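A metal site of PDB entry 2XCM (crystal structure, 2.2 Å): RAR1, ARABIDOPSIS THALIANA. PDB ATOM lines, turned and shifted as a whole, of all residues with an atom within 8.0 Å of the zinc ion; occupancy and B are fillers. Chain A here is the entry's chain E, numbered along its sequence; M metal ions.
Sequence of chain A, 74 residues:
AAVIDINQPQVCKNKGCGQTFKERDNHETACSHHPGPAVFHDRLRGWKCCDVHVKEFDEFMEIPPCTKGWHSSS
The side-chain sulfur (SG) of Cys 31 sits close to the side-chain amide nitrogen (ND2) of Asn 14 (3.3 Å).
N of Cys 31 sits at hydrogen-bond distance from O of Gly 69 (2.7 Å).
SG of Cys 12 sits close to ND2 of Asn 14, at 3.5 Å.
N of Ser 72 sits close to SG of Cys 12 (3.4 Å).
The backbone carbonyl oxygen (O) of Cys 12 lies close to the backbone NH (N) of Gly 18, 3.4 Å away.
NE2 of His 71 lies close to O of Ala 30 (3.4 Å).
The side-chain amide oxygen (OD1) of Asn 26 sits close to the backbone carbonyl oxygen (O) of His 71 (3.0 Å).
The side-chain sulfur (SG) of Cys 17 sits close to the backbone NH (N) of Gln 19 (3.4 Å).
Of the 21 residues printed, 4 come within 4 Å of the zinc ion.
The nearest printed residue that does not touch the zinc ion is Asn 14 (4.1 Å).
The zinc ion is bound by SG of Cys 31 (2.3 Å), SG of Cys 12 (2.3 Å), ND1 of His 71 (2.3 Å) and SG of Cys 17 (2.4 Å).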
ATOM      1  N   VAL A  11      -5.121 -28.167  20.129  1.00  0.00           N
ATOM      2  CA  VAL A  11      -4.353 -26.956  19.865  1.00  0.00           C
ATOM      3  C   VAL A  11      -5.125 -26.099  18.848  1.00  0.00           C
ATOM      4  O   VAL A  11      -5.496 -26.583  17.780  1.00  0.00           O
ATOM      5  CB  VAL A  11      -2.912 -27.269  19.359  1.00  0.00           C
ATOM      6  CG1 VAL A  11      -2.190 -25.987  18.963  1.00  0.00           C
ATOM      7  CG2 VAL A  11      -2.112 -27.995  20.448  1.00  0.00           C
ATOM      8  N   CYS A  12      -5.382 -24.853  19.194  1.00  0.00           N
ATOM      9  CA  CYS A  12      -6.070 -23.957  18.270  1.00  0.00           C
ATOM     10  C   CYS A  12      -5.115 -23.561  17.155  1.00  0.00           C
ATOM     11  O   CYS A  12      -3.964 -23.192  17.409  1.00  0.00           O
ATOM     12  CB  CYS A  12      -6.586 -22.712  18.998  1.00  0.00           C
ATOM     13  SG  CYS A  12      -7.494 -21.568  17.920  1.00  0.00           S
ATOM     14  N   LYS A  13      -5.587 -23.634  15.916  1.00  0.00           N
ATOM     15  CA  LYS A  13      -4.741 -23.352  14.778  1.00  0.00           C
ATOM     16  C   LYS A  13      -5.004 -21.977  14.166  1.00  0.00           C
ATOM     17  O   LYS A  13      -4.466 -21.648  13.115  1.00  0.00           O
ATOM     18  CB  LYS A  13      -4.894 -24.467  13.727  1.00  0.00           C
ATOM     19  CG  LYS A  13      -4.161 -25.753  14.113  1.00  0.00           C
ATOM     20  CD  LYS A  13      -5.084 -26.962  14.027  1.00  0.00           C
ATOM     21  CE  LYS A  13      -4.510 -28.148  14.823  1.00  0.00           C
ATOM     22  NZ  LYS A  13      -5.304 -29.389  14.561  1.00  0.00           N
ATOM     23  N   ASN A  14      -5.846 -21.175  14.815  1.00  0.00           N
ATOM     24  CA  ASN A  14      -6.077 -19.807  14.366  1.00  0.00           C
ATOM     25  C   ASN A  14      -4.819 -18.958  14.529  1.00  0.00           C
ATOM     26  O   ASN A  14      -4.112 -19.063  15.530  1.00  0.00           O
ATOM     27  CB  ASN A  14      -7.242 -19.170  15.147  1.00  0.00           C
ATOM     28  CG  ASN A  14      -8.581 -19.812  14.822  1.00  0.00           C
ATOM     29  OD1 ASN A  14      -8.770 -20.375  13.744  1.00  0.00           O
ATOM     30  ND2 ASN A  14      -9.523 -19.707  15.755  1.00  0.00           N
ATOM     31  N   LYS A  15      -4.558 -18.107  13.541  1.00  0.00           N
ATOM     32  CA  LYS A  15      -3.343 -17.291  13.531  1.00  0.00           C
ATOM     33  C   LYS A  15      -3.284 -16.316  14.710  1.00  0.00           C
ATOM     34  O   LYS A  15      -4.191 -15.487  14.896  1.00  0.00           O
ATOM     35  CB  LYS A  15      -3.210 -16.537  12.187  1.00  0.00           C
ATOM     36  CG  LYS A  15      -3.051 -17.444  10.930  1.00  0.00           C
ATOM     37  CD  LYS A  15      -3.121 -16.642   9.593  1.00  0.00           C
ATOM     38  CE  LYS A  15      -2.752 -17.489   8.349  1.00  0.00           C
ATOM     39  NZ  LYS A  15      -2.359 -16.701   7.078  1.00  0.00           N
ATOM     40  N   GLY A  16      -2.215 -16.424  15.503  1.00  0.00           N
ATOM     41  CA  GLY A  16      -2.031 -15.524  16.628  1.00  0.00           C
ATOM     42  C   GLY A  16      -2.579 -16.082  17.932  1.00  0.00           C
ATOM     43  O   GLY A  16      -2.488 -15.426  18.969  1.00  0.00           O
ATOM     44  N   CYS A  17      -3.135 -17.297  17.886  1.00  0.00           N
ATOM     45  CA  CYS A  17      -3.602 -17.977  19.100  1.00  0.00           C
ATOM     46  C   CYS A  17      -2.670 -19.136  19.467  1.00  0.00           C
ATOM     47  O   CYS A  17      -1.815 -18.986  20.341  1.00  0.00           O
ATOM     48  CB  CYS A  17      -5.039 -18.495  18.965  1.00  0.00           C
ATOM     49  SG  CYS A  17      -5.684 -19.353  20.490  1.00  0.00           S
ATOM     50  N   GLY A  18      -2.857 -20.285  18.826  1.00  0.00           N
ATOM     51  CA  GLY A  18      -2.073 -21.474  19.136  1.00  0.00           C
ATOM     52  C   GLY A  18      -2.250 -22.028  20.540  1.00  0.00           C
ATOM     53  O   GLY A  18      -1.465 -22.856  20.997  1.00  0.00           O
ATOM     54  N   GLN A  19      -3.277 -21.584  21.255  1.00  0.00           N
ATOM     55  CA  GLN A  19      -3.513 -22.082  22.610  1.00  0.00           C
ATOM     56  C   GLN A  19      -4.159 -23.464  22.672  1.00  0.00           C
ATOM     57  O   GLN A  19      -4.879 -23.884  21.760  1.00  0.00           O
ATOM     58  CB  GLN A  19      -4.330 -21.075  23.432  1.00  0.00           C
ATOM     59  CG  GLN A  19      -3.629 -19.737  23.574  1.00  0.00           C
ATOM     60  CD  GLN A  19      -4.414 -18.714  24.374  1.00  0.00           C
ATOM     61  OE1 GLN A  19      -5.359 -19.048  25.087  1.00  0.00           O
ATOM     62  NE2 GLN A  19      -4.010 -17.452  24.276  1.00  0.00           N
ATOM     63  N   THR A  20      -3.912 -24.161  23.764  1.00  0.00           N
ATOM     64  CA  THR A  20      -4.582 -25.421  24.048  1.00  0.00           C
ATOM     65  C   THR A  20      -5.922 -25.125  24.689  1.00  0.00           C
ATOM     66  O   THR A  20      -5.993 -24.373  25.647  1.00  0.00           O
ATOM     67  CB  THR A  20      -3.759 -26.286  25.013  1.00  0.00           C
ATOM     68  OG1 THR A  20      -2.575 -26.728  24.343  1.00  0.00           O
ATOM     69  CG2 THR A  20      -4.558 -27.503  25.475  1.00  0.00           C
ATOM     70  N   PHE A  21      -6.986 -25.723  24.151  1.00  0.00           N
ATOM     71  CA  PHE A  21      -8.343 -25.481  24.634  1.00  0.00           C
ATOM     72  C   PHE A  21      -9.194 -26.749  24.613  1.00  0.00           C
ATOM     73  O   PHE A  21      -8.886 -27.699  23.879  1.00  0.00           O
ATOM     74  CB  PHE A  21      -9.025 -24.414  23.778  1.00  0.00           C
ATOM     75  CG  PHE A  21      -9.461 -24.925  22.441  1.00  0.00           C
ATOM     76  CD1 PHE A  21     -10.796 -25.311  22.222  1.00  0.00           C
ATOM     77  CD2 PHE A  21      -8.574 -25.046  21.409  1.00  0.00           C
ATOM     78  CE1 PHE A  21     -11.214 -25.779  20.990  1.00  0.00           C
ATOM     79  CE2 PHE A  21      -8.984 -25.522  20.170  1.00  0.00           C
ATOM     80  CZ  PHE A  21     -10.314 -25.890  19.962  1.00  0.00           C
ATOM     81  N   ASN A  26     -15.127 -23.756  24.870  1.00  0.00           N
ATOM     82  CA  ASN A  26     -15.098 -22.913  23.678  1.00  0.00           C
ATOM     83  C   ASN A  26     -16.380 -22.081  23.555  1.00  0.00           C
ATOM     84  O   ASN A  26     -17.418 -22.452  24.095  1.00  0.00           O
ATOM     85  CB  ASN A  26     -14.915 -23.802  22.443  1.00  0.00           C
ATOM     86  CG  ASN A  26     -14.282 -23.055  21.251  1.00  0.00           C
ATOM     87  OD1 ASN A  26     -14.162 -23.620  20.168  1.00  0.00           O
ATOM     88  ND2 ASN A  26     -13.881 -21.807  21.455  1.00  0.00           N
ATOM     89  N   ALA A  30     -14.240 -16.630  22.262  1.00  0.00           N
ATOM     90  CA  ALA A  30     -13.135 -17.194  23.055  1.00  0.00           C
ATOM     91  C   ALA A  30     -11.722 -16.934  22.521  1.00  0.00           C
ATOM     92  O   ALA A  30     -10.774 -16.783  23.301  1.00  0.00           O
ATOM     93  CB  ALA A  30     -13.315 -18.690  23.230  1.00  0.00           C
ATOM     94  N   CYS A  31     -11.592 -16.876  21.200  1.00  0.00           N
ATOM     95  CA  CYS A  31     -10.281 -16.908  20.552  1.00  0.00           C
ATOM     96  C   CYS A  31      -9.922 -15.582  19.907  1.00  0.00           C
ATOM     97  O   CYS A  31     -10.614 -15.117  19.004  1.00  0.00           O
ATOM     98  CB  CYS A  31     -10.255 -18.001  19.496  1.00  0.00           C
ATOM     99  SG  CYS A  31      -8.695 -18.076  18.543  1.00  0.00           S
ATOM    100  N   SER A  32      -8.828 -14.954  20.339  1.00  0.00           N
ATOM    101  CA  SER A  32      -8.371 -13.765  19.639  1.00  0.00           C
ATOM    102  C   SER A  32      -7.288 -14.103  18.633  1.00  0.00           C
ATOM    103  O   SER A  32      -6.266 -14.697  18.994  1.00  0.00           O
ATOM    104  CB  SER A  32      -7.946 -12.649  20.600  1.00  0.00           C
ATOM    105  OG  SER A  32      -7.237 -13.185  21.682  1.00  0.00           O
ATOM    106  N   HIS A  33      -7.537 -13.734  17.385  1.00  0.00           N
ATOM    107  CA  HIS A  33      -6.734 -14.211  16.267  1.00  0.00           C
ATOM    108  C   HIS A  33      -6.941 -13.298  15.061  1.00  0.00           C
ATOM    109  O   HIS A  33      -7.899 -12.514  15.028  1.00  0.00           O
ATOM    110  CB  HIS A  33      -7.172 -15.630  15.917  1.00  0.00           C
ATOM    111  CG  HIS A  33      -8.601 -15.714  15.456  1.00  0.00           C
ATOM    112  ND1 HIS A  33      -8.950 -16.003  14.159  1.00  0.00           N
ATOM    113  CD2 HIS A  33      -9.756 -15.503  16.123  1.00  0.00           C
ATOM    114  CE1 HIS A  33     -10.272 -15.980  14.047  1.00  0.00           C
ATOM    115  NE2 HIS A  33     -10.780 -15.680  15.233  1.00  0.00           N
ATOM    116  N   GLY A  69     -13.279 -14.880  18.042  1.00  0.00           N
ATOM    117  CA  GLY A  69     -14.149 -15.902  17.490  1.00  0.00           C
ATOM    118  C   GLY A  69     -14.053 -17.197  18.289  1.00  0.00           C
ATOM    119  O   GLY A  69     -13.632 -17.186  19.458  1.00  0.00           O
ATOM    120  N   TRP A  70     -14.426 -18.305  17.642  1.00  0.00           N
ATOM    121  CA  TRP A  70     -14.256 -19.646  18.203  1.00  0.00           C
ATOM    122  C   TRP A  70     -12.812 -20.122  18.039  1.00  0.00           C
ATOM    123  O   TRP A  70     -12.219 -19.942  16.990  1.00  0.00           O
ATOM    124  CB  TRP A  70     -15.172 -20.661  17.486  1.00  0.00           C
ATOM    125  CG  TRP A  70     -16.663 -20.358  17.575  1.00  0.00           C
ATOM    126  CD1 TRP A  70     -17.375 -19.460  16.808  1.00  0.00           C
ATOM    127  CD2 TRP A  70     -17.613 -20.959  18.471  1.00  0.00           C
ATOM    128  NE1 TRP A  70     -18.691 -19.481  17.175  1.00  0.00           N
ATOM    129  CE2 TRP A  70     -18.868 -20.381  18.181  1.00  0.00           C
ATOM    130  CE3 TRP A  70     -17.521 -21.933  19.467  1.00  0.00           C
ATOM    131  CZ2 TRP A  70     -20.030 -20.746  18.878  1.00  0.00           C
ATOM    132  CZ3 TRP A  70     -18.668 -22.285  20.154  1.00  0.00           C
ATOM    133  CH2 TRP A  70     -19.914 -21.694  19.846  1.00  0.00           C
ATOM    134  N   HIS A  71     -12.254 -20.777  19.054  1.00  0.00           N
ATOM    135  CA  HIS A  71     -11.044 -21.542  18.837  1.00  0.00           C
ATOM    136  C   HIS A  71     -11.371 -22.596  17.786  1.00  0.00           C
ATOM    137  O   HIS A  71     -12.499 -23.079  17.725  1.00  0.00           O
ATOM    138  CB  HIS A  71     -10.594 -22.258  20.101  1.00  0.00           C
ATOM    139  CG  HIS A  71     -10.307 -21.336  21.252  1.00  0.00           C
ATOM    140  ND1 HIS A  71      -9.225 -20.480  21.259  1.00  0.00           N
ATOM    141  CD2 HIS A  71     -10.958 -21.144  22.420  1.00  0.00           C
ATOM    142  CE1 HIS A  71      -9.235 -19.786  22.390  1.00  0.00           C
ATOM    143  NE2 HIS A  71     -10.265 -20.177  23.109  1.00  0.00           N
ATOM    144  N   SER A  72     -10.389 -22.965  16.976  1.00  0.00           N
ATOM    145  CA  SER A  72     -10.595 -23.978  15.965  1.00  0.00           C
ATOM    146  C   SER A  72      -9.464 -25.017  15.948  1.00  0.00           C
ATOM    147  O   SER A  72      -8.308 -24.707  15.675  1.00  0.00           O
ATOM    148  CB  SER A  72     -10.745 -23.344  14.578  1.00  0.00           C
ATOM    149  OG  SER A  72     -10.941 -24.352  13.599  1.00  0.00           O
ATOM    150  N   SER A  73      -9.847 -26.258  16.220  1.00  0.00           N
ATOM    151  CA  SER A  73      -8.930 -27.382  16.213  1.00  0.00           C
ATOM    152  C   SER A  73      -8.457 -27.714  14.797  1.00  0.00           C
ATOM    153  O   SER A  73      -7.708 -28.650  14.589  1.00  0.00           O
ATOM    154  CB  SER A  73      -9.638 -28.602  16.833  1.00  0.00           C
ATOM    155  OG  SER A  73      -8.827 -29.755  16.776  1.00  0.00           O
HETATM  156 ZN    ZN M   1      -7.813 -19.925  19.508  1.00  0.00          ZN
